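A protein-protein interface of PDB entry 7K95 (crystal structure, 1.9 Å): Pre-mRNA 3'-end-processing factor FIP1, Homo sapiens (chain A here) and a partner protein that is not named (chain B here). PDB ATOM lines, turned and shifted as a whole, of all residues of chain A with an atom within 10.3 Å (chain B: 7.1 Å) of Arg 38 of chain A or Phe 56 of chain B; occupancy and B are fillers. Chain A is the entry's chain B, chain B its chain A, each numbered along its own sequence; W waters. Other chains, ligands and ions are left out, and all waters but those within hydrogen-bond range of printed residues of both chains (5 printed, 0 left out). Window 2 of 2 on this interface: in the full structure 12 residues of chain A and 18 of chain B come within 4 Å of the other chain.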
ATOM      1  N   TYR A  20     -16.260 -27.349   8.582  1.00  0.00           N
ATOM      2  CA  TYR A  20     -14.913 -27.186   7.968  1.00  0.00           C
ATOM      3  C   TYR A  20     -14.134 -26.005   8.553  1.00  0.00           C
ATOM      4  O   TYR A  20     -13.068 -25.722   7.986  1.00  0.00           O
ATOM      5  CB  TYR A  20     -14.992 -26.970   6.449  1.00  0.00           C
ATOM      6  CG  TYR A  20     -15.843 -28.043   5.830  1.00  0.00           C
ATOM      7  CD1 TYR A  20     -15.401 -29.331   5.829  1.00  0.00           C
ATOM      8  CD2 TYR A  20     -17.090 -27.786   5.312  1.00  0.00           C
ATOM      9  CE1 TYR A  20     -16.171 -30.332   5.328  1.00  0.00           C
ATOM     10  CE2 TYR A  20     -17.887 -28.793   4.804  1.00  0.00           C
ATOM     11  CZ  TYR A  20     -17.435 -30.077   4.849  1.00  0.00           C
ATOM     12  OH  TYR A  20     -18.183 -31.115   4.413  1.00  0.00           O
ATOM     13  N   PHE A  22     -15.328 -22.942   8.543  1.00  0.00           N
ATOM     14  CA  PHE A  22     -15.860 -21.708   7.913  1.00  0.00           C
ATOM     15  C   PHE A  22     -16.427 -20.745   8.972  1.00  0.00           C
ATOM     16  O   PHE A  22     -16.927 -21.181  10.036  1.00  0.00           O
ATOM     17  CB  PHE A  22     -16.991 -22.055   6.981  1.00  0.00           C
ATOM     18  CG  PHE A  22     -16.551 -22.543   5.629  1.00  0.00           C
ATOM     19  CD1 PHE A  22     -15.820 -21.716   4.794  1.00  0.00           C
ATOM     20  CD2 PHE A  22     -16.943 -23.790   5.161  1.00  0.00           C
ATOM     21  CE1 PHE A  22     -15.436 -22.148   3.531  1.00  0.00           C
ATOM     22  CE2 PHE A  22     -16.596 -24.198   3.893  1.00  0.00           C
ATOM     23  CZ  PHE A  22     -15.824 -23.393   3.099  1.00  0.00           C
ATOM     24  N   THR A  26     -15.922 -16.300   5.479  1.00  0.00           N
ATOM     25  CA  THR A  26     -15.210 -17.280   4.607  1.00  0.00           C
ATOM     26  C   THR A  26     -16.244 -18.102   3.831  1.00  0.00           C
ATOM     27  O   THR A  26     -16.018 -18.401   2.634  1.00  0.00           O
ATOM     28  CB  THR A  26     -14.200 -18.123   5.398  1.00  0.00           C
ATOM     29  OG1 THR A  26     -14.808 -18.823   6.482  1.00  0.00           O
ATOM     30  CG2 THR A  26     -13.030 -17.315   5.923  1.00  0.00           C
ATOM     31  N   TRP A  27     -17.417 -18.373   4.444  1.00  0.00           N
ATOM     32  CA  TRP A  27     -18.527 -19.071   3.769  1.00  0.00           C
ATOM     33  C   TRP A  27     -18.988 -18.238   2.560  1.00  0.00           C
ATOM     34  O   TRP A  27     -19.114 -18.769   1.429  1.00  0.00           O
ATOM     35  CB  TRP A  27     -19.674 -19.371   4.759  1.00  0.00           C
ATOM     36  CG  TRP A  27     -20.830 -20.022   4.065  1.00  0.00           C
ATOM     37  CD1 TRP A  27     -22.051 -19.475   3.776  1.00  0.00           C
ATOM     38  CD2 TRP A  27     -20.819 -21.313   3.426  1.00  0.00           C
ATOM     39  NE1 TRP A  27     -22.814 -20.357   3.049  1.00  0.00           N
ATOM     40  CE2 TRP A  27     -22.092 -21.506   2.851  1.00  0.00           C
ATOM     41  CE3 TRP A  27     -19.900 -22.363   3.388  1.00  0.00           C
ATOM     42  CZ2 TRP A  27     -22.427 -22.680   2.182  1.00  0.00           C
ATOM     43  CZ3 TRP A  27     -20.225 -23.511   2.694  1.00  0.00           C
ATOM     44  CH2 TRP A  27     -21.466 -23.658   2.086  1.00  0.00           C
ATOM     45  N   LYS A  28     -19.237 -16.943   2.755  1.00  0.00           N
ATOM     46  CA  LYS A  28     -19.677 -16.097   1.615  1.00  0.00           C
ATOM     47  C   LYS A  28     -18.610 -16.075   0.497  1.00  0.00           C
ATOM     48  O   LYS A  28     -18.951 -16.140  -0.710  1.00  0.00           O
ATOM     49  CB  LYS A  28     -19.960 -14.681   2.087  1.00  0.00           C
ATOM     50  CG  LYS A  28     -20.460 -13.775   0.977  1.00  0.00           C
ATOM     51  CD  LYS A  28     -21.021 -12.458   1.494  1.00  0.00           C
ATOM     52  CE  LYS A  28     -20.004 -11.334   1.495  1.00  0.00           C
ATOM     53  NZ  LYS A  28     -20.610 -10.073   1.983  1.00  0.00           N
ATOM     54  N   ALA A  29     -17.332 -16.016   0.847  1.00  0.00           N
ATOM     55  CA  ALA A  29     -16.246 -16.012  -0.172  1.00  0.00           C
ATOM     56  C   ALA A  29     -16.297 -17.334  -0.938  1.00  0.00           C
ATOM     57  O   ALA A  29     -16.217 -17.385  -2.205  1.00  0.00           O
ATOM     58  CB  ALA A  29     -14.897 -15.829   0.516  1.00  0.00           C
ATOM     59  N   TYR A  30     -16.429 -18.446  -0.194  1.00  0.00           N
ATOM     60  CA  TYR A  30     -16.504 -19.770  -0.845  1.00  0.00           C
ATOM     61  C   TYR A  30     -17.700 -19.862  -1.782  1.00  0.00           C
ATOM     62  O   TYR A  30     -17.530 -20.391  -2.913  1.00  0.00           O
ATOM     63  CB  TYR A  30     -16.562 -20.839   0.246  1.00  0.00           C
ATOM     64  CG  TYR A  30     -16.802 -22.243  -0.217  1.00  0.00           C
ATOM     65  CD1 TYR A  30     -15.761 -23.022  -0.740  1.00  0.00           C
ATOM     66  CD2 TYR A  30     -17.979 -22.871   0.079  1.00  0.00           C
ATOM     67  CE1 TYR A  30     -15.930 -24.371  -1.000  1.00  0.00           C
ATOM     68  CE2 TYR A  30     -18.172 -24.200  -0.228  1.00  0.00           C
ATOM     69  CZ  TYR A  30     -17.133 -24.980  -0.664  1.00  0.00           C
ATOM     70  OH  TYR A  30     -17.437 -26.272  -0.951  1.00  0.00           O
ATOM     71  N   CYS A  31     -18.858 -19.325  -1.389  1.00  0.00           N
ATOM     72  CA  CYS A  31     -20.041 -19.235  -2.292  1.00  0.00           C
ATOM     73  C   CYS A  31     -19.725 -18.429  -3.580  1.00  0.00           C
ATOM     74  O   CYS A  31     -20.135 -18.846  -4.653  1.00  0.00           O
ATOM     75  CB  CYS A  31     -21.281 -18.730  -1.565  1.00  0.00           C
ATOM     76  SG  CYS A  31     -21.818 -19.877  -0.255  1.00  0.00           S
ATOM     77  N   GLU A  32     -18.972 -17.348  -3.513  1.00  0.00           N
ATOM     78  CA  GLU A  32     -18.590 -16.530  -4.725  1.00  0.00           C
ATOM     79  C   GLU A  32     -17.574 -17.295  -5.606  1.00  0.00           C
ATOM     80  O   GLU A  32     -17.669 -17.303  -6.927  1.00  0.00           O
ATOM     81  CB  GLU A  32     -18.121 -15.196  -4.133  1.00  0.00           C
ATOM     82  CG  GLU A  32     -17.841 -14.133  -5.148  1.00  0.00           C
ATOM     83  CD  GLU A  32     -19.099 -13.817  -5.923  1.00  0.00           C
ATOM     84  OE1 GLU A  32     -20.187 -13.736  -5.266  1.00  0.00           O
ATOM     85  OE2 GLU A  32     -18.982 -13.763  -7.158  1.00  0.00           O
ATOM     86  N   LYS A  33     -16.650 -18.026  -4.958  1.00  0.00           N
ATOM     87  CA  LYS A  33     -15.669 -18.899  -5.683  1.00  0.00           C
ATOM     88  C   LYS A  33     -16.408 -19.980  -6.460  1.00  0.00           C
ATOM     89  O   LYS A  33     -16.076 -20.174  -7.645  1.00  0.00           O
ATOM     90  CB  LYS A  33     -14.617 -19.446  -4.727  1.00  0.00           C
ATOM     91  CG  LYS A  33     -13.808 -20.593  -5.320  1.00  0.00           C
ATOM     92  CD  LYS A  33     -12.850 -21.249  -4.348  1.00  0.00           C
ATOM     93  CE  LYS A  33     -11.738 -20.294  -3.945  1.00  0.00           C
ATOM     94  NZ  LYS A  33     -11.042 -20.806  -2.732  1.00  0.00           N
ATOM     95  N   GLN A  34     -17.367 -20.687  -5.817  1.00  0.00           N
ATOM     96  CA  GLN A  34     -18.204 -21.674  -6.539  1.00  0.00           C
ATOM     97  C   GLN A  34     -18.730 -21.034  -7.800  1.00  0.00           C
ATOM     98  O   GLN A  34     -18.745 -21.704  -8.851  1.00  0.00           O
ATOM     99  CB  GLN A  34     -19.343 -22.098  -5.628  1.00  0.00           C
ATOM    100  CG  GLN A  34     -18.875 -22.939  -4.471  1.00  0.00           C
ATOM    101  CD  GLN A  34     -18.702 -24.401  -4.781  1.00  0.00           C
ATOM    102  OE1 GLN A  34     -18.999 -24.882  -5.883  1.00  0.00           O
ATOM    103  NE2 GLN A  34     -18.144 -25.150  -3.808  1.00  0.00           N
ATOM    104  N   LYS A  35     -19.334 -19.855  -7.657  1.00  0.00           N
ATOM    105  CA  LYS A  35     -20.011 -19.181  -8.805  1.00  0.00           C
ATOM    106  C   LYS A  35     -18.985 -18.821  -9.885  1.00  0.00           C
ATOM    107  O   LYS A  35     -19.173 -19.177 -11.081  1.00  0.00           O
ATOM    108  CB  LYS A  35     -20.725 -17.894  -8.372  1.00  0.00           C
ATOM    109  CG  LYS A  35     -21.426 -17.083  -9.467  1.00  0.00           C
ATOM    110  CD  LYS A  35     -21.939 -15.695  -9.056  1.00  0.00           C
ATOM    111  CE  LYS A  35     -22.840 -15.733  -7.820  1.00  0.00           C
ATOM    112  NZ  LYS A  35     -23.648 -14.533  -7.502  1.00  0.00           N
ATOM    113  N   ARG A  36     -17.909 -18.190  -9.495  1.00  0.00           N
ATOM    114  CA  ARG A  36     -16.861 -17.816 -10.508  1.00  0.00           C
ATOM    115  C   ARG A  36     -16.325 -19.037 -11.296  1.00  0.00           C
ATOM    116  O   ARG A  36     -16.176 -18.978 -12.577  1.00  0.00           O
ATOM    117  CB  ARG A  36     -15.683 -17.156  -9.807  1.00  0.00           C
ATOM    118  CG  ARG A  36     -14.573 -16.716 -10.756  1.00  0.00           C
ATOM    119  CD  ARG A  36     -13.520 -15.899 -10.015  1.00  0.00           C
ATOM    120  NE  ARG A  36     -12.995 -16.653  -8.873  1.00  0.00           N
ATOM    121  CZ  ARG A  36     -12.156 -17.674  -8.969  1.00  0.00           C
ATOM    122  NH1 ARG A  36     -11.678 -18.047 -10.158  1.00  0.00           N
ATOM    123  NH2 ARG A  36     -11.770 -18.309  -7.871  1.00  0.00           N
ATOM    124  N   ILE A  37     -15.922 -20.098 -10.619  1.00  0.00           N
ATOM    125  CA  ILE A  37     -15.271 -21.249 -11.304  1.00  0.00           C
ATOM    126  C   ILE A  37     -16.349 -21.933 -12.147  1.00  0.00           C
ATOM    127  O   ILE A  37     -16.096 -22.229 -13.316  1.00  0.00           O
ATOM    128  CB  ILE A  37     -14.644 -22.180 -10.241  1.00  0.00           C
ATOM    129  CG1 ILE A  37     -13.559 -21.430  -9.464  1.00  0.00           C
ATOM    130  CG2 ILE A  37     -14.145 -23.465 -10.897  1.00  0.00           C
ATOM    131  CD1 ILE A  37     -12.864 -22.223  -8.389  1.00  0.00           C
ATOM    132  N   ARG A  38     -17.554 -22.152 -11.601  1.00  0.00           N
ATOM    133  CA  ARG A  38     -18.568 -23.009 -12.316  1.00  0.00           C
ATOM    134  C   ARG A  38     -19.053 -22.389 -13.628  1.00  0.00           C
ATOM    135  O   ARG A  38     -19.420 -23.186 -14.579  1.00  0.00           O
ATOM    136  CB  ARG A  38     -19.759 -23.345 -11.433  1.00  0.00           C
ATOM    137  CG  ARG A  38     -19.406 -24.377 -10.375  1.00  0.00           C
ATOM    138  CD  ARG A  38     -20.630 -24.466  -9.453  1.00  0.00           C
ATOM    139  NE  ARG A  38     -20.314 -25.278  -8.328  1.00  0.00           N
ATOM    140  CZ  ARG A  38     -20.356 -26.571  -8.287  1.00  0.00           C
ATOM    141  NH1 ARG A  38     -20.767 -27.250  -9.339  1.00  0.00           N
ATOM    142  NH2 ARG A  38     -19.879 -27.210  -7.206  1.00  0.00           N
ATOM    143  N   MET A  39     -19.089 -21.065 -13.707  1.00  0.00           N
ATOM    144  CA  MET A  39     -19.729 -20.415 -14.862  1.00  0.00           C
ATOM    145  C   MET A  39     -19.004 -20.808 -16.176  1.00  0.00           C
ATOM    146  O   MET A  39     -19.639 -20.852 -17.292  1.00  0.00           O
ATOM    147  CB  MET A  39     -19.683 -18.912 -14.626  1.00  0.00           C
ATOM    148  CG  MET A  39     -21.077 -18.448 -14.189  1.00  0.00           C
ATOM    149  SD  MET A  39     -20.837 -16.890 -13.530  1.00  0.00           S
ATOM    150  CE  MET A  39     -21.203 -15.965 -15.026  1.00  0.00           C
ATOM    151  N   GLY A  40     -17.695 -21.077 -16.087  1.00  0.00           N
ATOM    152  CA  GLY A  40     -16.861 -21.304 -17.282  1.00  0.00           C
ATOM    153  C   GLY A  40     -16.726 -22.775 -17.670  1.00  0.00           C
ATOM    154  O   GLY A  40     -15.835 -23.052 -18.523  1.00  0.00           O
ATOM    155  N   LEU A  41     -17.513 -23.686 -17.072  1.00  0.00           N
ATOM    156  CA  LEU A  41     -17.366 -25.169 -17.246  1.00  0.00           C
ATOM    157  C   LEU A  41     -18.622 -25.836 -17.860  1.00  0.00           C
ATOM    158  O   LEU A  41     -19.697 -25.212 -17.813  1.00  0.00           O
ATOM    159  CB  LEU A  41     -17.036 -25.783 -15.892  1.00  0.00           C
ATOM    160  CG  LEU A  41     -15.749 -25.255 -15.263  1.00  0.00           C
ATOM    161  CD1 LEU A  41     -15.567 -25.924 -13.920  1.00  0.00           C
ATOM    162  CD2 LEU A  41     -14.581 -25.552 -16.174  1.00  0.00           C
ATOM    163  N   GLU A  42     -18.445 -27.048 -18.436  1.00  0.00           N
ATOM    164  CA  GLU A  42     -19.378 -27.724 -19.381  1.00  0.00           C
ATOM    165  C   GLU A  42     -20.110 -28.884 -18.696  1.00  0.00           C
ATOM    166  O   GLU A  42     -20.736 -29.583 -19.569  1.00  0.00           O
ATOM    167  CB  GLU A  42     -18.601 -28.226 -20.604  1.00  0.00           C
ATOM    168  CG  GLU A  42     -17.624 -27.207 -21.168  1.00  0.00           C
ATOM    169  CD  GLU A  42     -16.833 -27.726 -22.348  1.00  0.00           C
ATOM    170  OE1 GLU A  42     -16.282 -28.844 -22.242  1.00  0.00           O
ATOM    171  OE2 GLU A  42     -16.820 -27.031 -23.377  1.00  0.00           O
ATOM    172  N   ARG B  16     -22.573 -29.674   3.250  1.00  0.00           N
ATOM    173  CA  ARG B  16     -22.251 -28.663   2.180  1.00  0.00           C
ATOM    174  C   ARG B  16     -21.471 -27.518   2.843  1.00  0.00           C
ATOM    175  O   ARG B  16     -20.468 -26.997   2.187  1.00  0.00           O
ATOM    176  CB  ARG B  16     -23.569 -28.196   1.534  1.00  0.00           C
ATOM    177  CG  ARG B  16     -23.421 -26.969   0.624  1.00  0.00           C
ATOM    178  CD  ARG B  16     -24.765 -26.677  -0.053  1.00  0.00           C
ATOM    179  NE  ARG B  16     -24.817 -25.534  -0.956  1.00  0.00           N
ATOM    180  CZ  ARG B  16     -25.111 -24.331  -0.582  1.00  0.00           C
ATOM    181  NH1 ARG B  16     -25.325 -24.089   0.700  1.00  0.00           N
ATOM    182  NH2 ARG B  16     -25.236 -23.348  -1.457  1.00  0.00           N
ATOM    183  N   GLY B  17     -21.767 -27.211   4.128  1.00  0.00           N
ATOM    184  CA  GLY B  17     -20.891 -26.338   4.940  1.00  0.00           C
ATOM    185  C   GLY B  17     -21.604 -25.383   5.881  1.00  0.00           C
ATOM    186  O   GLY B  17     -20.953 -24.850   6.827  1.00  0.00           O
ATOM    187  N   TYR B  38      -9.267 -30.985  -3.200  1.00  0.00           N
ATOM    188  CA  TYR B  38     -10.635 -30.857  -3.714  1.00  0.00           C
ATOM    189  C   TYR B  38     -11.068 -29.384  -3.695  1.00  0.00           C
ATOM    190  O   TYR B  38     -11.689 -28.938  -4.680  1.00  0.00           O
ATOM    191  CB  TYR B  38     -11.576 -31.759  -2.944  1.00  0.00           C
ATOM    192  CG  TYR B  38     -12.898 -31.979  -3.629  1.00  0.00           C
ATOM    193  CD1 TYR B  38     -12.975 -32.878  -4.680  1.00  0.00           C
ATOM    194  CD2 TYR B  38     -14.057 -31.295  -3.250  1.00  0.00           C
ATOM    195  CE1 TYR B  38     -14.179 -33.146  -5.336  1.00  0.00           C
ATOM    196  CE2 TYR B  38     -15.242 -31.562  -3.894  1.00  0.00           C
ATOM    197  CZ  TYR B  38     -15.322 -32.505  -4.900  1.00  0.00           C
ATOM    198  OH  TYR B  38     -16.521 -32.756  -5.506  1.00  0.00           O
ATOM    199  N   HIS B  53     -14.756 -34.164   0.613  1.00  0.00           N
ATOM    200  CA  HIS B  53     -14.998 -33.469  -0.682  1.00  0.00           C
ATOM    201  C   HIS B  53     -16.410 -32.892  -0.726  1.00  0.00           C
ATOM    202  O   HIS B  53     -17.340 -33.570  -1.138  1.00  0.00           O
ATOM    203  CB  HIS B  53     -14.720 -34.430  -1.809  1.00  0.00           C
ATOM    204  CG  HIS B  53     -13.302 -34.890  -1.958  1.00  0.00           C
ATOM    205  ND1 HIS B  53     -12.973 -35.818  -2.961  1.00  0.00           N
ATOM    206  CD2 HIS B  53     -12.178 -34.706  -1.219  1.00  0.00           C
ATOM    207  CE1 HIS B  53     -11.685 -36.127  -2.842  1.00  0.00           C
ATOM    208  NE2 HIS B  53     -11.206 -35.485  -1.778  1.00  0.00           N
ATOM    209  N   PRO B  54     -16.637 -31.687  -0.208  1.00  0.00           N
ATOM    210  CA  PRO B  54     -18.009 -31.201  -0.009  1.00  0.00           C
ATOM    211  C   PRO B  54     -18.649 -30.788  -1.327  1.00  0.00           C
ATOM    212  O   PRO B  54     -17.929 -30.098  -2.134  1.00  0.00           O
ATOM    213  CB  PRO B  54     -17.826 -29.983   0.881  1.00  0.00           C
ATOM    214  CG  PRO B  54     -16.420 -30.076   1.461  1.00  0.00           C
ATOM    215  CD  PRO B  54     -15.640 -30.824   0.415  1.00  0.00           C
ATOM    216  N   ARG B  55     -19.859 -31.268  -1.546  1.00  0.00           N
ATOM    217  CA  ARG B  55     -20.657 -30.907  -2.745  1.00  0.00           C
ATOM    218  C   ARG B  55     -21.338 -29.585  -2.479  1.00  0.00           C
ATOM    219  O   ARG B  55     -21.522 -29.193  -1.296  1.00  0.00           O
ATOM    220  CB  ARG B  55     -21.639 -31.996  -3.156  1.00  0.00           C
ATOM    221  CG  ARG B  55     -21.020 -33.374  -3.357  1.00  0.00           C
ATOM    222  CD  ARG B  55     -19.892 -33.421  -4.352  1.00  0.00           C
ATOM    223  NE  ARG B  55     -19.700 -34.757  -4.868  1.00  0.00           N
ATOM    224  CZ  ARG B  55     -18.858 -35.676  -4.432  1.00  0.00           C
ATOM    225  NH1 ARG B  55     -18.828 -36.865  -5.041  1.00  0.00           N
ATOM    226  NH2 ARG B  55     -18.014 -35.428  -3.440  1.00  0.00           N
ATOM    227  N   PHE B  56     -21.702 -28.859  -3.546  1.00  0.00           N
ATOM    228  CA  PHE B  56     -22.337 -27.551  -3.366  1.00  0.00           C
ATOM    229  C   PHE B  56     -23.830 -27.588  -3.719  1.00  0.00           C
ATOM    230  O   PHE B  56     -24.504 -26.556  -3.477  1.00  0.00           O
ATOM    231  CB  PHE B  56     -21.554 -26.496  -4.149  1.00  0.00           C
ATOM    232  CG  PHE B  56     -21.834 -25.102  -3.659  1.00  0.00           C
ATOM    233  CD1 PHE B  56     -21.433 -24.710  -2.380  1.00  0.00           C
ATOM    234  CD2 PHE B  56     -22.499 -24.190  -4.479  1.00  0.00           C
ATOM    235  CE1 PHE B  56     -21.658 -23.422  -1.942  1.00  0.00           C
ATOM    236  CE2 PHE B  56     -22.713 -22.903  -4.021  1.00  0.00           C
ATOM    237  CZ  PHE B  56     -22.326 -22.550  -2.763  1.00  0.00           C
ATOM    238  N   GLU B  57     -24.302 -28.597  -4.454  1.00  0.00           N
ATOM    239  CA  GLU B  57     -25.741 -28.824  -4.743  1.00  0.00           C
ATOM    240  C   GLU B  57     -26.573 -28.645  -3.469  1.00  0.00           C
ATOM    241  O   GLU B  57     -26.175 -29.176  -2.402  1.00  0.00           O
ATOM    242  CB  GLU B  57     -25.928 -30.210  -5.337  1.00  0.00           C
ATOM    243  CG  GLU B  57     -25.584 -30.305  -6.810  1.00  0.00           C
ATOM    244  CD  GLU B  57     -24.107 -30.415  -7.080  1.00  0.00           C
ATOM    245  OE1 GLU B  57     -23.359 -30.684  -6.084  1.00  0.00           O
ATOM    246  OE2 GLU B  57     -23.723 -30.198  -8.245  1.00  0.00           O
ATOM    247  N   LEU B  58     -27.664 -27.889  -3.514  1.00  0.00           N
ATOM    248  CA  LEU B  58     -28.495 -27.725  -2.307  1.00  0.00           C
ATOM    249  C   LEU B  58     -29.449 -28.908  -2.168  1.00  0.00           C
ATOM    250  O   LEU B  58     -30.157 -29.285  -3.097  1.00  0.00           O
ATOM    251  CB  LEU B  58     -29.312 -26.436  -2.397  1.00  0.00           C
ATOM    252  CG  LEU B  58     -28.584 -25.220  -1.879  1.00  0.00           C
ATOM    253  CD1 LEU B  58     -29.355 -23.993  -2.178  1.00  0.00           C
ATOM    254  CD2 LEU B  58     -28.328 -25.375  -0.358  1.00  0.00           C
ATOM    255  N   PRO B  59     -29.558 -29.463  -0.961  1.00  0.00           N
ATOM    256  CA  PRO B  59     -30.622 -30.404  -0.659  1.00  0.00           C
ATOM    257  C   PRO B  59     -31.947 -29.630  -0.588  1.00  0.00           C
ATOM    258  O   PRO B  59     -31.922 -28.435  -0.464  1.00  0.00           O
ATOM    259  CB  PRO B  59     -30.262 -30.969   0.720  1.00  0.00           C
ATOM    260  CG  PRO B  59     -28.981 -30.273   1.179  1.00  0.00           C
ATOM    261  CD  PRO B  59     -28.678 -29.160   0.179  1.00  0.00           C
HETATM  262  O   HOH W   1     -15.723 -28.285  -2.013  1.00  0.00           O
HETATM  263  O   HOH W   2     -19.798 -27.160  -0.342  1.00  0.00           O
HETATM  264  O   HOH W   3     -21.367 -30.183  -9.301  1.00  0.00           O
HETATM  265  O   HOH W   4     -20.780 -29.756  -6.134  1.00  0.00           O
HETATM  266  O   HOH W   5     -18.350 -28.080  -4.166  1.00  0.00           O
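Hydrophobic or aromatic side chains of chain B that line the printed part of chain A: Pro 54 and Phe 56.
Of the 19 printed residues of chain A, 6 touch a printed residue of chain B.
Among the printed residues, 8 pairs touch across the chains.
Among the printed residues, no Asp or Glu carboxylate lies within 4 Å of a Lys or Arg side-chain nitrogen of the other chain.
CA of Gly 17 of chain B touches CE2 of Tyr 20 of chain A, 3.9 Å away.
Tyr 20 of chain A touches Pro 54 of chain B.
Arg 16 of chain B touches Trp 27 of chain A (O to CH2, 3.5 Å).
Trp 27 of chain A touches Gly 17 of chain B.
Tyr 30 of chain A touches Phe 56 of chain B.
Cys 31 of chain A touches Phe 56 of chain B.
CD of Gln 34 of chain A touches CG of Phe 56 of chain B, at 3.4 Å.
Arg 38 of chain A touches Phe 56 of chain B.
The side-chain hydroxyl (OH) of Tyr 30 of chain A sits at hydrogen-bond distance from the side-chain amide nitrogen (NE2) of Gln 34 of chain A (3.1 Å).
The guanidinium group (NE) of Arg 16 of chain B is in hydrogen-bond range of the backbone carbonyl oxygen (O) of Phe 56 of chain B (2.7 Å).
The side-chain amide oxygen (OE1) of Gln 34 of chain A lies within hydrogen-bond range of the guanidinium group (NE) of Arg 38 of chain A, 2.8 Å away.
The side-chain sulfur (SG) of Cys 31 of chain A is in hydrogen-bond range of the backbone carbonyl oxygen (O) of Trp 27 of chain A (3.4 Å).
Phe 56 of chain B touches four residues of chain A.
No residue of chain A comes within 4 Å of Glu 57 of chain B.
Of the printed residues of chain A, Arg 16 of chain B touches Trp 27 (3.5 Å).
Of the printed residues of chain B, Tyr 30 of chain A touches Phe 56.
Of the printed residues of chain B, Trp 27 of chain A touches Arg 16 (3.5 Å) and Gly 17 (3.7 Å).
Printed residues of chain B within 4 Å of Gln 34 of chain A: Phe 56 (3.4 Å).
The nearest residue of chain B that does not touch Arg 38 of chain A is Glu 57 of chain B (4.3 Å).
The nearest residue of chain A that does not touch Phe 56 of chain B is Trp 27 of chain A (4.04 Å).
Water W3 lies within hydrogen-bond range of OE2 of Glu 57 of chain B (2.6 Å) and NH1 of Arg 38 of chain A (3.0 Å).
Water W2 lies within hydrogen-bond range of OH of Tyr 30 of chain A (2.6 Å), O of Arg 16 of chain B (2.6 Å) and O of Arg 55 of chain B (2.8 Å).
Water W4 lies within hydrogen-bond range of the side-chain carboxylate of Glu 57 of chain B, the backbone NH of Phe 56 of chain B and the guanidinium group of Arg 38 of chain A.
Water W1 bridges OH of Tyr 30 of chain A and O of Pro 54 of chain B.
Water W5 lies within hydrogen-bond range of O of Pro 54 of chain B (2.9 Å), NE2 of Gln 34 of chain A (3.0 Å) and N of Phe 56 of chain B (3.5 Å).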
